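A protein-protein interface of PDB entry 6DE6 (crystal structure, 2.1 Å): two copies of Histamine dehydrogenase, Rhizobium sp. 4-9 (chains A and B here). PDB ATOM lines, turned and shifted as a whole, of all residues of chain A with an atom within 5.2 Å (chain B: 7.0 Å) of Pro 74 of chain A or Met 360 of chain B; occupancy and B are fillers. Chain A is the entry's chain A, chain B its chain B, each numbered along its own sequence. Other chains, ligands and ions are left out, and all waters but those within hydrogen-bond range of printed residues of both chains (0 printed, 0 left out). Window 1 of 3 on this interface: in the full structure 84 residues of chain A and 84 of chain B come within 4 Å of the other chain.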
ATOM      1  N   ILE A  72     -11.162  -3.278 -18.253  1.00  0.00           N
ATOM      2  CA  ILE A  72      -9.858  -3.140 -18.886  1.00  0.00           C
ATOM      3  C   ILE A  72      -9.185  -4.483 -19.147  1.00  0.00           C
ATOM      4  O   ILE A  72      -7.948  -4.572 -19.154  1.00  0.00           O
ATOM      5  CB  ILE A  72      -8.918  -2.246 -18.039  1.00  0.00           C
ATOM      6  CG1 ILE A  72      -8.767  -2.782 -16.611  1.00  0.00           C
ATOM      7  CG2 ILE A  72      -9.404  -0.783 -18.005  1.00  0.00           C
ATOM      8  CD1 ILE A  72      -7.627  -2.104 -15.836  1.00  0.00           C
ATOM      9  N   THR A  73      -9.977  -5.527 -19.340  1.00  0.00           N
ATOM     10  CA  THR A  73      -9.469  -6.810 -19.810  1.00  0.00           C
ATOM     11  C   THR A  73      -8.489  -6.518 -20.939  1.00  0.00           C
ATOM     12  O   THR A  73      -8.787  -5.692 -21.804  1.00  0.00           O
ATOM     13  CB  THR A  73     -10.614  -7.714 -20.305  1.00  0.00           C
ATOM     14  OG1 THR A  73     -11.477  -8.081 -19.211  1.00  0.00           O
ATOM     15  CG2 THR A  73     -10.080  -8.988 -20.986  1.00  0.00           C
ATOM     16  N   PRO A  74      -7.329  -7.176 -20.996  1.00  0.00           N
ATOM     17  CA  PRO A  74      -6.866  -8.349 -20.251  1.00  0.00           C
ATOM     18  C   PRO A  74      -6.376  -8.113 -18.815  1.00  0.00           C
ATOM     19  O   PRO A  74      -6.138  -9.101 -18.133  1.00  0.00           O
ATOM     20  CB  PRO A  74      -5.692  -8.850 -21.110  1.00  0.00           C
ATOM     21  CG  PRO A  74      -5.156  -7.617 -21.765  1.00  0.00           C
ATOM     22  CD  PRO A  74      -6.344  -6.724 -21.996  1.00  0.00           C
ATOM     23  N   PHE A  75      -6.258  -6.872 -18.346  1.00  0.00           N
ATOM     24  CA  PHE A  75      -5.718  -6.662 -17.009  1.00  0.00           C
ATOM     25  C   PHE A  75      -6.633  -7.308 -15.989  1.00  0.00           C
ATOM     26  O   PHE A  75      -7.854  -7.234 -16.111  1.00  0.00           O
ATOM     27  CB  PHE A  75      -5.542  -5.168 -16.699  1.00  0.00           C
ATOM     28  CG  PHE A  75      -4.408  -4.554 -17.418  1.00  0.00           C
ATOM     29  CD1 PHE A  75      -3.141  -4.594 -16.873  1.00  0.00           C
ATOM     30  CD2 PHE A  75      -4.600  -3.923 -18.646  1.00  0.00           C
ATOM     31  CE1 PHE A  75      -2.073  -4.027 -17.549  1.00  0.00           C
ATOM     32  CE2 PHE A  75      -3.548  -3.367 -19.314  1.00  0.00           C
ATOM     33  CZ  PHE A  75      -2.278  -3.419 -18.764  1.00  0.00           C
ATOM     34  N   ILE A  76      -6.031  -7.954 -14.984  1.00  0.00           N
ATOM     35  CA  ILE A  76      -6.766  -8.676 -13.953  1.00  0.00           C
ATOM     36  C   ILE A  76      -6.650  -7.895 -12.659  1.00  0.00           C
ATOM     37  O   ILE A  76      -5.671  -8.016 -11.915  1.00  0.00           O
ATOM     38  CB  ILE A  76      -6.258 -10.108 -13.760  1.00  0.00           C
ATOM     39  CG1 ILE A  76      -6.478 -10.945 -15.025  1.00  0.00           C
ATOM     40  CG2 ILE A  76      -6.948 -10.731 -12.539  1.00  0.00           C
ATOM     41  CD1 ILE A  76      -5.806 -12.327 -14.939  1.00  0.00           C
ATOM     42  N   PHE A 117     -13.337  -5.170 -23.862  1.00  0.00           N
ATOM     43  CA  PHE A 117     -13.124  -6.320 -24.725  1.00  0.00           C
ATOM     44  C   PHE A 117     -13.890  -7.543 -24.238  1.00  0.00           C
ATOM     45  O   PHE A 117     -14.329  -8.359 -25.058  1.00  0.00           O
ATOM     46  CB  PHE A 117     -11.636  -6.639 -24.806  1.00  0.00           C
ATOM     47  CG  PHE A 117     -10.888  -5.776 -25.766  1.00  0.00           C
ATOM     48  CD1 PHE A 117     -11.378  -5.541 -27.042  1.00  0.00           C
ATOM     49  CD2 PHE A 117      -9.692  -5.215 -25.400  1.00  0.00           C
ATOM     50  CE1 PHE A 117     -10.673  -4.737 -27.939  1.00  0.00           C
ATOM     51  CE2 PHE A 117      -8.973  -4.435 -26.283  1.00  0.00           C
ATOM     52  CZ  PHE A 117      -9.468  -4.182 -27.550  1.00  0.00           C
ATOM     53  N   MET A 360      -0.269 -10.340 -16.154  1.00  0.00           N
ATOM     54  CA  MET A 360      -1.445 -11.015 -15.588  1.00  0.00           C
ATOM     55  C   MET A 360      -1.085 -12.349 -14.934  1.00  0.00           C
ATOM     56  O   MET A 360      -1.752 -13.371 -15.156  1.00  0.00           O
ATOM     57  CB  MET A 360      -2.518 -11.233 -16.655  1.00  0.00           C
ATOM     58  CG  MET A 360      -3.002  -9.971 -17.356  1.00  0.00           C
ATOM     59  SD  MET A 360      -2.081  -9.535 -18.850  1.00  0.00           S
ATOM     60  CE  MET A 360      -2.299  -7.752 -18.854  1.00  0.00           C
ATOM     61  N   GLY B  35     -10.865 -17.364 -26.393  1.00  0.00           N
ATOM     62  CA  GLY B  35     -10.819 -16.279 -25.425  1.00  0.00           C
ATOM     63  C   GLY B  35     -11.529 -16.530 -24.102  1.00  0.00           C
ATOM     64  O   GLY B  35     -11.648 -15.595 -23.297  1.00  0.00           O
ATOM     65  N   GLY B  36     -12.049 -17.740 -23.873  1.00  0.00           N
ATOM     66  CA  GLY B  36     -12.713 -18.096 -22.628  1.00  0.00           C
ATOM     67  C   GLY B  36     -11.873 -19.067 -21.817  1.00  0.00           C
ATOM     68  O   GLY B  36     -11.518 -18.771 -20.671  1.00  0.00           O
ATOM     69  N   ARG B  39     -11.084 -19.660 -17.778  1.00  0.00           N
ATOM     70  CA  ARG B  39     -11.808 -18.595 -17.077  1.00  0.00           C
ATOM     71  C   ARG B  39     -13.315 -18.659 -17.319  1.00  0.00           C
ATOM     72  O   ARG B  39     -14.097 -18.416 -16.396  1.00  0.00           O
ATOM     73  CB  ARG B  39     -11.293 -17.211 -17.505  1.00  0.00           C
ATOM     74  CG  ARG B  39     -11.953 -16.020 -16.755  1.00  0.00           C
ATOM     75  CD  ARG B  39     -11.551 -14.692 -17.390  1.00  0.00           C
ATOM     76  NE  ARG B  39     -11.876 -14.701 -18.815  1.00  0.00           N
ATOM     77  CZ  ARG B  39     -11.302 -13.941 -19.745  1.00  0.00           C
ATOM     78  NH1 ARG B  39     -10.349 -13.069 -19.427  1.00  0.00           N
ATOM     79  NH2 ARG B  39     -11.685 -14.056 -21.009  1.00  0.00           N
ATOM     80  N   ASP B  40     -13.748 -18.939 -18.552  1.00  0.00           N
ATOM     81  CA  ASP B  40     -15.164 -18.905 -18.915  1.00  0.00           C
ATOM     82  C   ASP B  40     -15.595 -20.277 -19.429  1.00  0.00           C
ATOM     83  O   ASP B  40     -16.041 -20.412 -20.572  1.00  0.00           O
ATOM     84  CB  ASP B  40     -15.407 -17.822 -19.961  1.00  0.00           C
ATOM     85  CG  ASP B  40     -14.809 -16.482 -19.555  1.00  0.00           C
ATOM     86  OD1 ASP B  40     -15.324 -15.870 -18.584  1.00  0.00           O
ATOM     87  OD2 ASP B  40     -13.815 -16.056 -20.197  1.00  0.00           O
ATOM     88  N   ILE B  72       1.746 -20.527 -20.407  1.00  0.00           N
ATOM     89  CA  ILE B  72       2.018 -19.370 -21.235  1.00  0.00           C
ATOM     90  C   ILE B  72       1.183 -18.175 -20.811  1.00  0.00           C
ATOM     91  O   ILE B  72       0.834 -17.331 -21.648  1.00  0.00           O
ATOM     92  CB  ILE B  72       1.778 -19.691 -22.718  1.00  0.00           C
ATOM     93  CG1 ILE B  72       0.356 -20.209 -22.937  1.00  0.00           C
ATOM     94  CG2 ILE B  72       2.799 -20.701 -23.240  1.00  0.00           C
ATOM     95  CD1 ILE B  72      -0.025 -20.231 -24.402  1.00  0.00           C
ATOM     96  N   THR B  73       0.831 -18.111 -19.531  1.00  0.00           N
ATOM     97  CA  THR B  73       0.195 -16.924 -18.967  1.00  0.00           C
ATOM     98  C   THR B  73       0.973 -15.723 -19.492  1.00  0.00           C
ATOM     99  O   THR B  73       2.210 -15.736 -19.475  1.00  0.00           O
ATOM    100  CB  THR B  73       0.205 -16.976 -17.433  1.00  0.00           C
ATOM    101  OG1 THR B  73      -0.515 -18.124 -17.003  1.00  0.00           O
ATOM    102  CG2 THR B  73      -0.490 -15.751 -16.810  1.00  0.00           C
ATOM    103  N   PRO B  74       0.309 -14.644 -19.931  1.00  0.00           N
ATOM    104  CA  PRO B  74      -1.103 -14.273 -19.796  1.00  0.00           C
ATOM    105  C   PRO B  74      -2.105 -14.942 -20.747  1.00  0.00           C
ATOM    106  O   PRO B  74      -3.304 -14.731 -20.591  1.00  0.00           O
ATOM    107  CB  PRO B  74      -1.076 -12.763 -20.033  1.00  0.00           C
ATOM    108  CG  PRO B  74       0.124 -12.547 -20.957  1.00  0.00           C
ATOM    109  CD  PRO B  74       1.125 -13.589 -20.570  1.00  0.00           C
ATOM    110  N   PHE B  75      -1.661 -15.727 -21.711  1.00  0.00           N
ATOM    111  CA  PHE B  75      -2.636 -16.359 -22.587  1.00  0.00           C
ATOM    112  C   PHE B  75      -3.523 -17.304 -21.784  1.00  0.00           C
ATOM    113  O   PHE B  75      -3.056 -18.008 -20.882  1.00  0.00           O
ATOM    114  CB  PHE B  75      -1.930 -17.092 -23.720  1.00  0.00           C
ATOM    115  CG  PHE B  75      -1.303 -16.161 -24.723  1.00  0.00           C
ATOM    116  CD1 PHE B  75      -2.035 -15.693 -25.811  1.00  0.00           C
ATOM    117  CD2 PHE B  75      -0.011 -15.718 -24.553  1.00  0.00           C
ATOM    118  CE1 PHE B  75      -1.474 -14.817 -26.726  1.00  0.00           C
ATOM    119  CE2 PHE B  75       0.567 -14.832 -25.473  1.00  0.00           C
ATOM    120  CZ  PHE B  75      -0.171 -14.382 -26.553  1.00  0.00           C
ATOM    121  N   ILE B  76      -4.820 -17.290 -22.090  1.00  0.00           N
ATOM    122  CA  ILE B  76      -5.804 -18.108 -21.392  1.00  0.00           C
ATOM    123  C   ILE B  76      -6.246 -19.208 -22.340  1.00  0.00           C
ATOM    124  O   ILE B  76      -7.127 -18.999 -23.183  1.00  0.00           O
ATOM    125  CB  ILE B  76      -7.020 -17.306 -20.931  1.00  0.00           C
ATOM    126  CG1 ILE B  76      -6.631 -16.239 -19.919  1.00  0.00           C
ATOM    127  CG2 ILE B  76      -8.078 -18.255 -20.335  1.00  0.00           C
ATOM    128  CD1 ILE B  76      -7.775 -15.312 -19.602  1.00  0.00           C
ATOM    129  N   ILE B 354      -8.932 -14.238 -33.570  1.00  0.00           N
ATOM    130  CA  ILE B 354      -7.608 -14.355 -32.963  1.00  0.00           C
ATOM    131  C   ILE B 354      -7.353 -13.220 -31.976  1.00  0.00           C
ATOM    132  O   ILE B 354      -6.700 -13.432 -30.945  1.00  0.00           O
ATOM    133  CB  ILE B 354      -6.526 -14.401 -34.066  1.00  0.00           C
ATOM    134  CG1 ILE B 354      -6.707 -15.655 -34.935  1.00  0.00           C
ATOM    135  CG2 ILE B 354      -5.093 -14.369 -33.460  1.00  0.00           C
ATOM    136  CD1 ILE B 354      -5.703 -15.764 -36.075  1.00  0.00           C
ATOM    137  N   THR B 355      -7.875 -12.010 -32.247  1.00  0.00           N
ATOM    138  CA  THR B 355      -7.618 -10.888 -31.345  1.00  0.00           C
ATOM    139  C   THR B 355      -8.192 -11.157 -29.958  1.00  0.00           C
ATOM    140  O   THR B 355      -7.636 -10.685 -28.959  1.00  0.00           O
ATOM    141  CB  THR B 355      -8.188  -9.564 -31.905  1.00  0.00           C
ATOM    142  OG1 THR B 355      -9.621  -9.540 -31.799  1.00  0.00           O
ATOM    143  CG2 THR B 355      -7.789  -9.352 -33.373  1.00  0.00           C
ATOM    144  N   GLY B 356      -9.281 -11.937 -29.875  1.00  0.00           N
ATOM    145  CA  GLY B 356      -9.852 -12.280 -28.584  1.00  0.00           C
ATOM    146  C   GLY B 356      -8.956 -13.176 -27.747  1.00  0.00           C
ATOM    147  O   GLY B 356      -8.985 -13.110 -26.513  1.00  0.00           O
ATOM    148  N   ASP B 357      -8.173 -14.041 -28.394  1.00  0.00           N
ATOM    149  CA  ASP B 357      -7.185 -14.839 -27.673  1.00  0.00           C
ATOM    150  C   ASP B 357      -5.958 -14.003 -27.300  1.00  0.00           C
ATOM    151  O   ASP B 357      -5.379 -14.176 -26.218  1.00  0.00           O
ATOM    152  CB  ASP B 357      -6.797 -16.057 -28.516  1.00  0.00           C
ATOM    153  CG  ASP B 357      -5.839 -16.999 -27.787  1.00  0.00           C
ATOM    154  OD1 ASP B 357      -6.326 -17.799 -26.952  1.00  0.00           O
ATOM    155  OD2 ASP B 357      -4.616 -16.944 -28.058  1.00  0.00           O
ATOM    156  N   MET B 358      -5.552 -13.095 -28.189  1.00  0.00           N
ATOM    157  CA  MET B 358      -4.400 -12.234 -27.941  1.00  0.00           C
ATOM    158  C   MET B 358      -4.692 -11.147 -26.908  1.00  0.00           C
ATOM    159  O   MET B 358      -3.748 -10.589 -26.337  1.00  0.00           O
ATOM    160  CB  MET B 358      -3.949 -11.590 -29.256  1.00  0.00           C
ATOM    161  CG  MET B 358      -3.475 -12.604 -30.293  1.00  0.00           C
ATOM    162  SD  MET B 358      -1.827 -13.245 -29.934  1.00  0.00           S
ATOM    163  CE  MET B 358      -0.857 -11.753 -30.228  1.00  0.00           C
ATOM    164  N   THR B 359      -5.966 -10.826 -26.658  1.00  0.00           N
ATOM    165  CA  THR B 359      -6.341  -9.871 -25.617  1.00  0.00           C
ATOM    166  C   THR B 359      -7.092 -10.535 -24.465  1.00  0.00           C
ATOM    167  O   THR B 359      -7.613  -9.826 -23.594  1.00  0.00           O
ATOM    168  CB  THR B 359      -7.191  -8.730 -26.196  1.00  0.00           C
ATOM    169  OG1 THR B 359      -8.444  -9.248 -26.678  1.00  0.00           O
ATOM    170  CG2 THR B 359      -6.442  -8.002 -27.333  1.00  0.00           C
ATOM    171  N   MET B 360      -7.150 -11.876 -24.445  1.00  0.00           N
ATOM    172  CA  MET B 360      -7.690 -12.660 -23.324  1.00  0.00           C
ATOM    173  C   MET B 360      -9.095 -12.206 -22.919  1.00  0.00           C
ATOM    174  O   MET B 360      -9.365 -11.959 -21.740  1.00  0.00           O
ATOM    175  CB  MET B 360      -6.753 -12.596 -22.117  1.00  0.00           C
ATOM    176  CG  MET B 360      -5.336 -13.079 -22.382  1.00  0.00           C
ATOM    177  SD  MET B 360      -4.239 -11.756 -22.926  1.00  0.00           S
ATOM    178  CE  MET B 360      -2.990 -12.636 -23.859  1.00  0.00           C
ATOM    179  N   SER B 361     -10.011 -12.116 -23.915  1.00  0.00           N
ATOM    180  CA  SER B 361     -11.255 -11.371 -23.739  1.00  0.00           C
ATOM    181  C   SER B 361     -12.511 -12.002 -24.369  1.00  0.00           C
ATOM    182  O   SER B 361     -13.528 -11.308 -24.531  1.00  0.00           O
ATOM    183  CB  SER B 361     -11.062  -9.974 -24.324  1.00  0.00           C
ATOM    184  OG  SER B 361     -10.809 -10.033 -25.725  1.00  0.00           O
ATOM    185  N   ILE B 362     -12.485 -13.287 -24.715  1.00  0.00           N
ATOM    186  CA  ILE B 362     -13.603 -13.977 -25.370  1.00  0.00           C
ATOM    187  C   ILE B 362     -13.772 -13.469 -26.802  1.00  0.00           C
ATOM    188  O   ILE B 362     -14.100 -12.297 -27.053  1.00  0.00           O
ATOM    189  CB  ILE B 362     -14.923 -13.852 -24.579  1.00  0.00           C
ATOM    190  CG1 ILE B 362     -14.793 -14.523 -23.200  1.00  0.00           C
ATOM    191  CG2 ILE B 362     -16.040 -14.525 -25.370  1.00  0.00           C
ATOM    192  CD1 ILE B 362     -16.052 -14.451 -22.340  1.00  0.00           C
ATOM    193  N   SER B 363     -13.557 -14.371 -27.747  1.00  0.00           N
ATOM    194  CA  SER B 363     -13.409 -13.992 -29.137  1.00  0.00           C
ATOM    195  C   SER B 363     -14.749 -13.598 -29.749  1.00  0.00           C
ATOM    196  O   SER B 363     -15.809 -14.080 -29.353  1.00  0.00           O
ATOM    197  CB  SER B 363     -12.807 -15.142 -29.942  1.00  0.00           C
ATOM    198  OG  SER B 363     -11.542 -15.534 -29.460  1.00  0.00           O
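O of Phe 117 of chain A lies close to O of Ser 361 of chain B (3.1 Å).
The side-chain hydroxyl of Thr 359 of chain B is in hydrogen-bond range of the side-chain hydroxyl of Ser 361 of chain B, at 2.7 Å. O of Met 360 of chain B sits at hydrogen-bond distance from NH1 of Arg 39 of chain B (2.7 Å). The backbone carbonyl oxygen (O) of Gly 356 of chain B sits at hydrogen-bond distance from the backbone NH (N) of Ser 361 of chain B, 3.0 Å away. OG1 of Thr 359 of chain B sits at hydrogen-bond distance from O of Thr 355 of chain B (2.8 Å).
Among the printed residues, pairs that only touch across the chains: Thr 73 of chain A with Thr 359 of chain B (3.7 Å), Thr 73 of chain A with Met 360 of chain B (3.1 Å), Thr 73 of chain A with Ser 361 of chain B (3.6 Å), Pro 74 of chain A with Thr 359 of chain B (3.3 Å), Pro 74 of chain A with Met 360 of chain B (3.7 Å), Met 360 of chain A with Thr 73 of chain B (3.2 Å) and Met 360 of chain A with Pro 74 of chain B (3.6 Å).
Of the printed residues of chain B, Thr 73 of chain A touches Thr 359 (3.7 Å), Met 360 (3.1 Å) and Ser 361 (3.6 Å). Of chain B, only Thr 359 and Met 360 come within 4 Å of Pro 74 of chain A. Of the printed residues of chain A, Thr 73 of chain B touches Met 360 (3.2 Å). Of the printed residues of chain A, Pro 74 of chain B touches Met 360. Printed residues of chain A within 4 Å of Thr 359 of chain B: Thr 73 and Pro 74. Met 360 of chain B touches just these residues of chain A: Thr 73 (3.1 Å) and Pro 74 (3.7 Å). Printed residues of chain A within 4 Å of Ser 361 of chain B: Thr 73 (3.6 Å) and Phe 117 (3.1 Å). The nearest residue of chain B that does not touch Pro 74 of chain A is Met 358 of chain B (5.6 Å). The nearest residue of chain A that does not touch Met 360 of chain B is Met 360 of chain A (5.1 Å).
Hydrophobic or aromatic side chains of chain B within 4 Å of the printed part of chain A: Pro 74 and Met 360. Among the printed residues, 8 pairs touch across the chains. Among the printed residues, no Asp or Glu carboxylate lies within 4 Å of a Lys or Arg side-chain nitrogen of the other chain.
Thr 73 of chain A touches Met 360 of chain B, and with the chains exchanged Met 360 of chain A touches Thr 73 of chain B. Pro 74 of chain A touches Met 360 of chain B, and with the chains exchanged Met 360 of chain A touches Pro 74 of chain B. Positions printed for both chains: 72, 73, 74, 75, 76 and 360. Of the 8 pairs that touch across the chains among the printed residues, 4 have their exchanged pair printed and touching as well.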
